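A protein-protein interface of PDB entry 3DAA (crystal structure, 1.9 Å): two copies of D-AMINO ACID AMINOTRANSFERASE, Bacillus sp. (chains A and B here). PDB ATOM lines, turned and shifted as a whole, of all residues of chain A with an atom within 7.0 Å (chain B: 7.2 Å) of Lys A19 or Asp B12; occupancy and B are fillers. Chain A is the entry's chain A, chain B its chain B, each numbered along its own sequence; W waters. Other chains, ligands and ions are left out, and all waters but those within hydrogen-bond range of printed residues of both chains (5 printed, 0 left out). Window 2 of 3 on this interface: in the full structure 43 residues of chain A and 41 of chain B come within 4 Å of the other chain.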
ATOM      1  N   ILE A  17     -26.196  -1.924  29.008  1.00  0.00           N
ATOM      2  CA  ILE A  17     -25.076  -2.149  29.924  1.00  0.00           C
ATOM      3  C   ILE A  17     -24.253  -3.380  29.533  1.00  0.00           C
ATOM      4  O   ILE A  17     -24.817  -4.405  29.167  1.00  0.00           O
ATOM      5  CB  ILE A  17     -25.615  -2.315  31.382  1.00  0.00           C
ATOM      6  CG1 ILE A  17     -26.525  -1.132  31.762  1.00  0.00           C
ATOM      7  CG2 ILE A  17     -24.475  -2.493  32.372  1.00  0.00           C
ATOM      8  CD1 ILE A  17     -25.935   0.271  31.536  1.00  0.00           C
ATOM      9  N   ASP A  18     -22.927  -3.281  29.607  1.00  0.00           N
ATOM     10  CA  ASP A  18     -22.067  -4.421  29.266  1.00  0.00           C
ATOM     11  C   ASP A  18     -22.050  -5.448  30.405  1.00  0.00           C
ATOM     12  O   ASP A  18     -21.972  -5.074  31.576  1.00  0.00           O
ATOM     13  CB  ASP A  18     -20.635  -3.959  28.960  1.00  0.00           C
ATOM     14  CG  ASP A  18     -19.818  -5.018  28.215  1.00  0.00           C
ATOM     15  OD1 ASP A  18     -19.298  -5.954  28.855  1.00  0.00           O
ATOM     16  OD2 ASP A  18     -19.688  -4.906  26.978  1.00  0.00           O
ATOM     17  N   LYS A  19     -22.094  -6.735  30.049  1.00  0.00           N
ATOM     18  CA  LYS A  19     -22.094  -7.827  31.026  1.00  0.00           C
ATOM     19  C   LYS A  19     -20.851  -7.794  31.916  1.00  0.00           C
ATOM     20  O   LYS A  19     -20.846  -8.365  33.015  1.00  0.00           O
ATOM     21  CB  LYS A  19     -22.191  -9.190  30.320  1.00  0.00           C
ATOM     22  CG  LYS A  19     -20.974  -9.547  29.458  1.00  0.00           C
ATOM     23  CD  LYS A  19     -21.140 -10.888  28.758  1.00  0.00           C
ATOM     24  CE  LYS A  19     -19.870 -11.311  28.016  1.00  0.00           C
ATOM     25  NZ  LYS A  19     -19.478 -10.359  26.946  1.00  0.00           N
ATOM     26  N   GLU A  20     -19.796  -7.145  31.420  1.00  0.00           N
ATOM     27  CA  GLU A  20     -18.544  -7.020  32.162  1.00  0.00           C
ATOM     28  C   GLU A  20     -18.347  -5.657  32.827  1.00  0.00           C
ATOM     29  O   GLU A  20     -17.225  -5.270  33.158  1.00  0.00           O
ATOM     30  CB  GLU A  20     -17.334  -7.426  31.302  1.00  0.00           C
ATOM     31  CG  GLU A  20     -17.264  -8.937  31.058  1.00  0.00           C
ATOM     32  CD  GLU A  20     -15.909  -9.410  30.547  1.00  0.00           C
ATOM     33  OE1 GLU A  20     -15.431  -8.880  29.527  1.00  0.00           O
ATOM     34  OE2 GLU A  20     -15.321 -10.322  31.166  1.00  0.00           O
ATOM     35  N   ASP A  21     -19.449  -4.919  32.989  1.00  0.00           N
ATOM     36  CA  ASP A  21     -19.429  -3.634  33.693  1.00  0.00           C
ATOM     37  C   ASP A  21     -19.201  -4.116  35.132  1.00  0.00           C
ATOM     38  O   ASP A  21     -19.876  -5.044  35.586  1.00  0.00           O
ATOM     39  CB  ASP A  21     -20.804  -2.947  33.589  1.00  0.00           C
ATOM     40  CG  ASP A  21     -20.816  -1.537  34.167  1.00  0.00           C
ATOM     41  OD1 ASP A  21     -20.310  -1.342  35.288  1.00  0.00           O
ATOM     42  OD2 ASP A  21     -21.362  -0.618  33.511  1.00  0.00           O
ATOM     43  N   ARG A  22     -18.204  -3.560  35.814  1.00  0.00           N
ATOM     44  CA  ARG A  22     -17.903  -3.975  37.189  1.00  0.00           C
ATOM     45  C   ARG A  22     -19.048  -3.732  38.168  1.00  0.00           C
ATOM     46  O   ARG A  22     -19.069  -4.313  39.250  1.00  0.00           O
ATOM     47  CB  ARG A  22     -16.600  -3.330  37.680  1.00  0.00           C
ATOM     48  CG  ARG A  22     -15.370  -3.874  36.953  1.00  0.00           C
ATOM     49  CD  ARG A  22     -14.090  -3.141  37.317  1.00  0.00           C
ATOM     50  NE  ARG A  22     -13.726  -3.289  38.729  1.00  0.00           N
ATOM     51  CZ  ARG A  22     -12.907  -4.220  39.212  1.00  0.00           C
ATOM     52  NH1 ARG A  22     -12.359  -5.113  38.398  1.00  0.00           N
ATOM     53  NH2 ARG A  22     -12.597  -4.226  40.508  1.00  0.00           N
ATOM     54  N   TYR A  24     -22.019  -4.548  37.456  1.00  0.00           N
ATOM     55  CA  TYR A  24     -22.890  -5.695  37.234  1.00  0.00           C
ATOM     56  C   TYR A  24     -22.289  -7.001  37.780  1.00  0.00           C
ATOM     57  O   TYR A  24     -23.023  -7.933  38.125  1.00  0.00           O
ATOM     58  CB  TYR A  24     -23.183  -5.816  35.733  1.00  0.00           C
ATOM     59  CG  TYR A  24     -24.344  -6.712  35.376  1.00  0.00           C
ATOM     60  CD1 TYR A  24     -25.619  -6.484  35.899  1.00  0.00           C
ATOM     61  CD2 TYR A  24     -24.183  -7.763  34.473  1.00  0.00           C
ATOM     62  CE1 TYR A  24     -26.701  -7.279  35.525  1.00  0.00           C
ATOM     63  CE2 TYR A  24     -25.252  -8.559  34.095  1.00  0.00           C
ATOM     64  CZ  TYR A  24     -26.506  -8.314  34.620  1.00  0.00           C
ATOM     65  OH  TYR A  24     -27.561  -9.106  34.239  1.00  0.00           O
ATOM     66  N   GLN A  25     -20.962  -7.079  37.858  1.00  0.00           N
ATOM     67  CA  GLN A  25     -20.316  -8.290  38.370  1.00  0.00           C
ATOM     68  C   GLN A  25     -19.823  -8.198  39.818  1.00  0.00           C
ATOM     69  O   GLN A  25     -19.654  -9.222  40.489  1.00  0.00           O
ATOM     70  CB  GLN A  25     -19.145  -8.700  37.470  1.00  0.00           C
ATOM     71  CG  GLN A  25     -19.543  -9.010  36.032  1.00  0.00           C
ATOM     72  CD  GLN A  25     -18.413  -9.639  35.238  1.00  0.00           C
ATOM     73  OE1 GLN A  25     -17.310  -9.080  35.142  1.00  0.00           O
ATOM     74  NE2 GLN A  25     -18.682 -10.805  34.655  1.00  0.00           N
ATOM     75  N   THR A  95     -16.071  -0.943  32.481  1.00  0.00           N
ATOM     76  CA  THR A  95     -16.096  -2.265  31.850  1.00  0.00           C
ATOM     77  C   THR A  95     -14.706  -2.767  31.477  1.00  0.00           C
ATOM     78  O   THR A  95     -13.934  -2.054  30.833  1.00  0.00           O
ATOM     79  CB  THR A  95     -16.956  -2.244  30.562  1.00  0.00           C
ATOM     80  OG1 THR A  95     -18.305  -1.904  30.895  1.00  0.00           O
ATOM     81  CG2 THR A  95     -16.938  -3.609  29.878  1.00  0.00           C
ATOM     82  N   SER A  96     -14.398  -3.997  31.882  1.00  0.00           N
ATOM     83  CA  SER A  96     -13.114  -4.630  31.573  1.00  0.00           C
ATOM     84  C   SER A  96     -13.184  -6.111  31.902  1.00  0.00           C
ATOM     85  O   SER A  96     -14.056  -6.539  32.664  1.00  0.00           O
ATOM     86  CB  SER A  96     -11.953  -3.967  32.343  1.00  0.00           C
ATOM     87  OG  SER A  96     -12.078  -4.120  33.742  1.00  0.00           O
ATOM     88  N   GLY B   1     -17.256 -13.519  20.729  1.00  0.00           N
ATOM     89  CA  GLY B   1     -17.679 -14.944  20.750  1.00  0.00           C
ATOM     90  C   GLY B   1     -19.173 -15.099  20.949  1.00  0.00           C
ATOM     91  O   GLY B   1     -19.966 -14.313  20.421  1.00  0.00           O
ATOM     92  N   TYR B   2     -19.554 -16.128  21.702  1.00  0.00           N
ATOM     93  CA  TYR B   2     -20.954 -16.405  22.002  1.00  0.00           C
ATOM     94  C   TYR B   2     -21.228 -16.278  23.496  1.00  0.00           C
ATOM     95  O   TYR B   2     -20.412 -16.687  24.325  1.00  0.00           O
ATOM     96  CB  TYR B   2     -21.357 -17.790  21.486  1.00  0.00           C
ATOM     97  CG  TYR B   2     -21.429 -17.848  19.975  1.00  0.00           C
ATOM     98  CD1 TYR B   2     -22.593 -17.474  19.299  1.00  0.00           C
ATOM     99  CD2 TYR B   2     -20.313 -18.218  19.217  1.00  0.00           C
ATOM    100  CE1 TYR B   2     -22.641 -17.458  17.900  1.00  0.00           C
ATOM    101  CE2 TYR B   2     -20.348 -18.207  17.820  1.00  0.00           C
ATOM    102  CZ  TYR B   2     -21.514 -17.824  17.169  1.00  0.00           C
ATOM    103  OH  TYR B   2     -21.545 -17.797  15.789  1.00  0.00           O
ATOM    104  N   THR B   3     -22.388 -15.707  23.822  1.00  0.00           N
ATOM    105  CA  THR B   3     -22.812 -15.475  25.203  1.00  0.00           C
ATOM    106  C   THR B   3     -24.137 -16.170  25.519  1.00  0.00           C
ATOM    107  O   THR B   3     -25.065 -16.142  24.707  1.00  0.00           O
ATOM    108  CB  THR B   3     -23.006 -13.945  25.462  1.00  0.00           C
ATOM    109  OG1 THR B   3     -21.748 -13.267  25.358  1.00  0.00           O
ATOM    110  CG2 THR B   3     -23.600 -13.682  26.846  1.00  0.00           C
ATOM    111  N   LEU B   4     -24.215 -16.804  26.690  1.00  0.00           N
ATOM    112  CA  LEU B   4     -25.451 -17.447  27.127  1.00  0.00           C
ATOM    113  C   LEU B   4     -26.339 -16.321  27.648  1.00  0.00           C
ATOM    114  O   LEU B   4     -25.941 -15.571  28.539  1.00  0.00           O
ATOM    115  CB  LEU B   4     -25.192 -18.466  28.247  1.00  0.00           C
ATOM    116  CG  LEU B   4     -26.394 -18.934  29.095  1.00  0.00           C
ATOM    117  CD1 LEU B   4     -27.448 -19.598  28.220  1.00  0.00           C
ATOM    118  CD2 LEU B   4     -25.941 -19.876  30.207  1.00  0.00           C
ATOM    119  N   VAL B  10     -26.301 -16.609  22.009  1.00  0.00           N
ATOM    120  CA  VAL B  10     -26.203 -15.591  20.967  1.00  0.00           C
ATOM    121  C   VAL B  10     -24.820 -14.960  20.880  1.00  0.00           C
ATOM    122  O   VAL B  10     -23.929 -15.284  21.663  1.00  0.00           O
ATOM    123  CB  VAL B  10     -27.257 -14.462  21.203  1.00  0.00           C
ATOM    124  CG1 VAL B  10     -28.644 -15.068  21.407  1.00  0.00           C
ATOM    125  CG2 VAL B  10     -26.871 -13.600  22.404  1.00  0.00           C
ATOM    126  N   LYS B  11     -24.648 -14.064  19.912  1.00  0.00           N
ATOM    127  CA  LYS B  11     -23.385 -13.355  19.747  1.00  0.00           C
ATOM    128  C   LYS B  11     -23.298 -12.248  20.799  1.00  0.00           C
ATOM    129  O   LYS B  11     -24.304 -11.623  21.139  1.00  0.00           O
ATOM    130  CB  LYS B  11     -23.285 -12.764  18.345  1.00  0.00           C
ATOM    131  CG  LYS B  11     -23.215 -13.818  17.264  1.00  0.00           C
ATOM    132  CD  LYS B  11     -23.279 -13.195  15.887  1.00  0.00           C
ATOM    133  CE  LYS B  11     -22.124 -12.240  15.655  1.00  0.00           C
ATOM    134  NZ  LYS B  11     -22.245 -11.576  14.331  1.00  0.00           N
ATOM    135  N   ASP B  12     -22.087 -12.013  21.295  1.00  0.00           N
ATOM    136  CA  ASP B  12     -21.817 -11.007  22.325  1.00  0.00           C
ATOM    137  C   ASP B  12     -22.543  -9.668  22.177  1.00  0.00           C
ATOM    138  O   ASP B  12     -23.001  -9.092  23.157  1.00  0.00           O
ATOM    139  CB  ASP B  12     -20.306 -10.740  22.414  1.00  0.00           C
ATOM    140  CG  ASP B  12     -19.523 -11.905  23.021  1.00  0.00           C
ATOM    141  OD1 ASP B  12     -20.068 -13.028  23.120  1.00  0.00           O
ATOM    142  OD2 ASP B  12     -18.351 -11.689  23.406  1.00  0.00           O
ATOM    143  N   GLU B  13     -22.657  -9.188  20.945  1.00  0.00           N
ATOM    144  CA  GLU B  13     -23.284  -7.902  20.680  1.00  0.00           C
ATOM    145  C   GLU B  13     -24.810  -7.894  20.664  1.00  0.00           C
ATOM    146  O   GLU B  13     -25.420  -6.830  20.670  1.00  0.00           O
ATOM    147  CB  GLU B  13     -22.754  -7.323  19.361  1.00  0.00           C
ATOM    148  CG  GLU B  13     -21.225  -7.210  19.266  1.00  0.00           C
ATOM    149  CD  GLU B  13     -20.531  -8.544  18.989  1.00  0.00           C
ATOM    150  OE1 GLU B  13     -21.119  -9.408  18.293  1.00  0.00           O
ATOM    151  OE2 GLU B  13     -19.387  -8.720  19.465  1.00  0.00           O
ATOM    152  N   GLU B  14     -25.421  -9.070  20.664  1.00  0.00           N
ATOM    153  CA  GLU B  14     -26.880  -9.175  20.631  1.00  0.00           C
ATOM    154  C   GLU B  14     -27.534  -9.170  22.027  1.00  0.00           C
ATOM    155  O   GLU B  14     -28.758  -9.208  22.151  1.00  0.00           O
ATOM    156  CB  GLU B  14     -27.261 -10.437  19.852  1.00  0.00           C
ATOM    157  CG  GLU B  14     -28.672 -10.450  19.295  1.00  0.00           C
ATOM    158  CD  GLU B  14     -28.846 -11.469  18.176  1.00  0.00           C
ATOM    159  OE1 GLU B  14     -28.762 -12.688  18.447  1.00  0.00           O
ATOM    160  OE2 GLU B  14     -29.064 -11.044  17.019  1.00  0.00           O
ATOM    161  N   VAL B  15     -26.711  -9.088  23.069  1.00  0.00           N
ATOM    162  CA  VAL B  15     -27.182  -9.089  24.455  1.00  0.00           C
ATOM    163  C   VAL B  15     -27.513  -7.689  24.973  1.00  0.00           C
ATOM    164  O   VAL B  15     -26.701  -6.770  24.855  1.00  0.00           O
ATOM    165  CB  VAL B  15     -26.131  -9.729  25.371  1.00  0.00           C
ATOM    166  CG1 VAL B  15     -26.553  -9.618  26.826  1.00  0.00           C
ATOM    167  CG2 VAL B  15     -25.927 -11.179  24.977  1.00  0.00           C
ATOM    168  N   LYS B  16     -28.698  -7.540  25.566  1.00  0.00           N
ATOM    169  CA  LYS B  16     -29.134  -6.248  26.093  1.00  0.00           C
ATOM    170  C   LYS B  16     -29.419  -6.266  27.593  1.00  0.00           C
ATOM    171  O   LYS B  16     -30.434  -6.814  28.033  1.00  0.00           O
ATOM    172  CB  LYS B  16     -30.391  -5.755  25.359  1.00  0.00           C
ATOM    173  CG  LYS B  16     -30.299  -5.762  23.833  1.00  0.00           C
ATOM    174  CD  LYS B  16     -29.182  -4.866  23.321  1.00  0.00           C
ATOM    175  CE  LYS B  16     -29.104  -4.877  21.799  1.00  0.00           C
ATOM    176  NZ  LYS B  16     -28.093  -3.890  21.310  1.00  0.00           N
ATOM    177  N   ILE B  17     -28.524  -5.659  28.371  1.00  0.00           N
ATOM    178  CA  ILE B  17     -28.698  -5.575  29.818  1.00  0.00           C
ATOM    179  C   ILE B  17     -29.305  -4.210  30.128  1.00  0.00           C
ATOM    180  O   ILE B  17     -28.784  -3.175  29.698  1.00  0.00           O
ATOM    181  CB  ILE B  17     -27.372  -5.684  30.596  1.00  0.00           C
ATOM    182  CG1 ILE B  17     -26.615  -6.954  30.205  1.00  0.00           C
ATOM    183  CG2 ILE B  17     -27.664  -5.706  32.097  1.00  0.00           C
ATOM    184  CD1 ILE B  17     -27.371  -8.225  30.487  1.00  0.00           C
ATOM    185  N   ASN B  80     -17.972 -21.729  21.455  1.00  0.00           N
ATOM    186  CA  ASN B  80     -16.818 -20.856  21.631  1.00  0.00           C
ATOM    187  C   ASN B  80     -15.501 -21.566  21.375  1.00  0.00           C
ATOM    188  O   ASN B  80     -14.457 -20.921  21.338  1.00  0.00           O
ATOM    189  CB  ASN B  80     -16.805 -20.229  23.032  1.00  0.00           C
ATOM    190  CG  ASN B  80     -17.773 -19.067  23.165  1.00  0.00           C
ATOM    191  OD1 ASN B  80     -17.537 -17.980  22.636  1.00  0.00           O
ATOM    192  ND2 ASN B  80     -18.867 -19.291  23.877  1.00  0.00           N
ATOM    193  N   TYR B  88     -18.050 -18.425  33.030  1.00  0.00           N
ATOM    194  CA  TYR B  88     -18.583 -17.590  34.100  1.00  0.00           C
ATOM    195  C   TYR B  88     -20.077 -17.485  33.844  1.00  0.00           C
ATOM    196  O   TYR B  88     -20.478 -17.207  32.718  1.00  0.00           O
ATOM    197  CB  TYR B  88     -17.966 -16.185  34.091  1.00  0.00           C
ATOM    198  CG  TYR B  88     -18.667 -15.225  35.044  1.00  0.00           C
ATOM    199  CD1 TYR B  88     -19.810 -14.529  34.650  1.00  0.00           C
ATOM    200  CD2 TYR B  88     -18.219 -15.056  36.349  1.00  0.00           C
ATOM    201  CE1 TYR B  88     -20.493 -13.699  35.534  1.00  0.00           C
ATOM    202  CE2 TYR B  88     -18.896 -14.226  37.242  1.00  0.00           C
ATOM    203  CZ  TYR B  88     -20.030 -13.552  36.827  1.00  0.00           C
ATOM    204  OH  TYR B  88     -20.702 -12.727  37.704  1.00  0.00           O
ATOM    205  N   GLN B  90     -24.054 -16.238  35.721  1.00  0.00           N
ATOM    206  CA  GLN B  90     -24.805 -15.591  36.802  1.00  0.00           C
ATOM    207  C   GLN B  90     -26.290 -15.444  36.503  1.00  0.00           C
ATOM    208  O   GLN B  90     -26.723 -15.560  35.353  1.00  0.00           O
ATOM    209  CB  GLN B  90     -24.222 -14.190  37.094  1.00  0.00           C
ATOM    210  CG  GLN B  90     -24.297 -13.181  35.920  1.00  0.00           C
ATOM    211  CD  GLN B  90     -23.906 -11.750  36.309  1.00  0.00           C
ATOM    212  OE1 GLN B  90     -22.726 -11.407  36.369  1.00  0.00           O
ATOM    213  NE2 GLN B  90     -24.906 -10.905  36.555  1.00  0.00           N
ATOM    214  N   ILE B 112     -26.878 -14.805  32.447  1.00  0.00           N
ATOM    215  CA  ILE B 112     -25.763 -14.423  31.585  1.00  0.00           C
ATOM    216  C   ILE B 112     -24.592 -15.384  31.818  1.00  0.00           C
ATOM    217  O   ILE B 112     -24.224 -15.662  32.958  1.00  0.00           O
ATOM    218  CB  ILE B 112     -25.292 -12.972  31.901  1.00  0.00           C
ATOM    219  CG1 ILE B 112     -26.355 -11.959  31.468  1.00  0.00           C
ATOM    220  CG2 ILE B 112     -23.956 -12.670  31.223  1.00  0.00           C
ATOM    221  CD1 ILE B 112     -26.546 -11.878  29.970  1.00  0.00           C
ATOM    222  N   GLY B 113     -24.007 -15.888  30.735  1.00  0.00           N
ATOM    223  CA  GLY B 113     -22.880 -16.797  30.852  1.00  0.00           C
ATOM    224  C   GLY B 113     -21.942 -16.653  29.670  1.00  0.00           C
ATOM    225  O   GLY B 113     -22.395 -16.420  28.548  1.00  0.00           O
ATOM    226  N   TYR B 114     -20.641 -16.773  29.913  1.00  0.00           N
ATOM    227  CA  TYR B 114     -19.655 -16.659  28.840  1.00  0.00           C
ATOM    228  C   TYR B 114     -18.359 -17.389  29.169  1.00  0.00           C
ATOM    229  O   TYR B 114     -18.123 -17.747  30.319  1.00  0.00           O
ATOM    230  CB  TYR B 114     -19.372 -15.185  28.506  1.00  0.00           C
ATOM    231  CG  TYR B 114     -18.715 -14.376  29.607  1.00  0.00           C
ATOM    232  CD1 TYR B 114     -19.473 -13.826  30.647  1.00  0.00           C
ATOM    233  CD2 TYR B 114     -17.347 -14.106  29.576  1.00  0.00           C
ATOM    234  CE1 TYR B 114     -18.884 -13.019  31.626  1.00  0.00           C
ATOM    235  CE2 TYR B 114     -16.746 -13.303  30.550  1.00  0.00           C
ATOM    236  CZ  TYR B 114     -17.524 -12.762  31.568  1.00  0.00           C
ATOM    237  OH  TYR B 114     -16.942 -11.953  32.513  1.00  0.00           O
ATOM    238  N   THR B 115     -17.511 -17.585  28.160  1.00  0.00           N
ATOM    239  CA  THR B 115     -16.248 -18.297  28.347  1.00  0.00           C
ATOM    240  C   THR B 115     -15.012 -17.408  28.278  1.00  0.00           C
ATOM    241  O   THR B 115     -15.082 -16.256  27.849  1.00  0.00           O
ATOM    242  CB  THR B 115     -16.095 -19.435  27.320  1.00  0.00           C
ATOM    243  OG1 THR B 115     -16.021 -18.882  26.000  1.00  0.00           O
ATOM    244  CG2 THR B 115     -17.271 -20.400  27.405  1.00  0.00           C
HETATM  245  O   HOH W   1     -18.959 -11.761  39.483  1.00  0.00           O
HETATM  246  O   HOH W   2     -16.844 -11.391  26.238  1.00  0.00           O
HETATM  247  O   HOH W   3     -21.678 -10.800  33.784  1.00  0.00           O
HETATM  248  O   HOH W   4     -27.438 -11.915  34.862  1.00  0.00           O
HETATM  249  O   HOH W   5     -26.338  -5.127  27.092  1.00  0.00           O
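Of the printed residues of chain B, Ile A17 touches Ile B17.
Printed residues of chain B within 4 Å of Lys A19: Thr B3 (3.8 Å), Asp B12 (3.9 Å) and Tyr B114 (3.6 Å).
Of the printed residues of chain B, Glu A20 touches Tyr B114 (2.7 Å).
Of the printed residues of chain B, Tyr A24 touches Ile B17 (3.8 Å) and Gln B90 (3.4 Å).
Ser A96 touches none of the printed residues of chain B.
Of the printed residues of chain A, Thr B3 touches Lys A19 (3.8 Å).
Printed residues of chain A within 4 Å of Gln B90: Tyr A24 (3.4 Å) and Gln A25 (3.999 Å).
The nearest printed residue of chain B that does not touch Lys A19 is Ile B112 (4.01 Å).
The nearest residue of chain A that does not touch Asp B12 is Asp A18 (6.6 Å).
The nearest printed residue of chain A that does not touch Tyr B88 is Tyr A24 (5.3 Å).
Lys A19 touches Thr B3 (CE to OG1, 3.8 Å).
Tyr B114 touches Lys A19 (CG to CE, 3.6 Å).
CZ of Tyr A24 touches CG2 of Ile B17 (3.8 Å).
Tyr A24 touches Gln B90 (CE2 to NE2, 3.4 Å).
Gln A25 touches Tyr B88 (NE2 to CE1, 3.5 Å).
OE1 of Gln B90 touches CG of Gln A25 (3.999 Å).
Water W5 lies within hydrogen-bond range of the backbone NH of Ile B17 (2.6 Å), the backbone carbonyl oxygen of Ile A17 (2.7 Å) and the backbone carbonyl oxygen of Val B15 (2.8 Å).
Water W1 lies within hydrogen-bond range of OH of Tyr B88 and O of Gln A25.
Water W3 lies within hydrogen-bond range of O of Lys A19, OE1 of Gln B90 and NE2 of Gln A25.
Water W4 bridges OH of Tyr A24 and NE2 of Gln B90.
Water W2 bridges NZ of Lys A19 (2.9 Å) and OD2 of Asp B12 (3.2 Å).
Hydrophobic or aromatic side chains of chain A that line the printed part of chain B: Ile A17 and Tyr A24.
Hydrophobic or aromatic side chains of chain B within 4 Å of the printed part of chain A: Ile B17, Tyr B88 and Tyr B114.
Among the printed residues, 10 pairs touch across the chains.
Among the printed residues, Asp or Glu carboxylates within 4 Å of a Lys or Arg side-chain nitrogen of the other chain: Lys A19 with Asp B12 (3.9 Å).
The backbone NH (N) of Asp B12 is in hydrogen-bond range of the backbone carbonyl oxygen (O) of Gly B1, 3.2 Å away.
N of Thr B3 sits at hydrogen-bond distance from O of Val B10.
The side-chain carboxylate (OD1) of Asp B12 sits at hydrogen-bond distance from the side-chain hydroxyl (OG1) of Thr B3, at 2.8 Å.
The side-chain hydroxyl (OH) of Tyr B88 lies within hydrogen-bond range of the side-chain amide oxygen (OE1) of Gln B90 (2.8 Å).
The backbone NH (N) of Tyr B88 lies within hydrogen-bond range of the backbone carbonyl oxygen (O) of Tyr B114 (2.8 Å).
The backbone carbonyl oxygen of Ile B112 sits at hydrogen-bond distance from the backbone NH of Gln B90 (2.8 Å).
Ile B17 touches its own counterpart, Ile A17.
Position printed for both chains: 17.
The backbone NH (N) of Ile A17 sits at hydrogen-bond distance from the backbone carbonyl oxygen (O) of Ile B17.
NZ of Lys A19 lies within salt-bridge range of OD2 of Asp B12 (3.9 Å).
The side-chain hydroxyl (OH) of Tyr B114 lies within hydrogen-bond range of the side-chain carboxylate (OE2) of Glu A20, at 2.7 Å.
NE2 of Gln A25 is in hydrogen-bond range of OH of Tyr B114 (3.0 Å).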
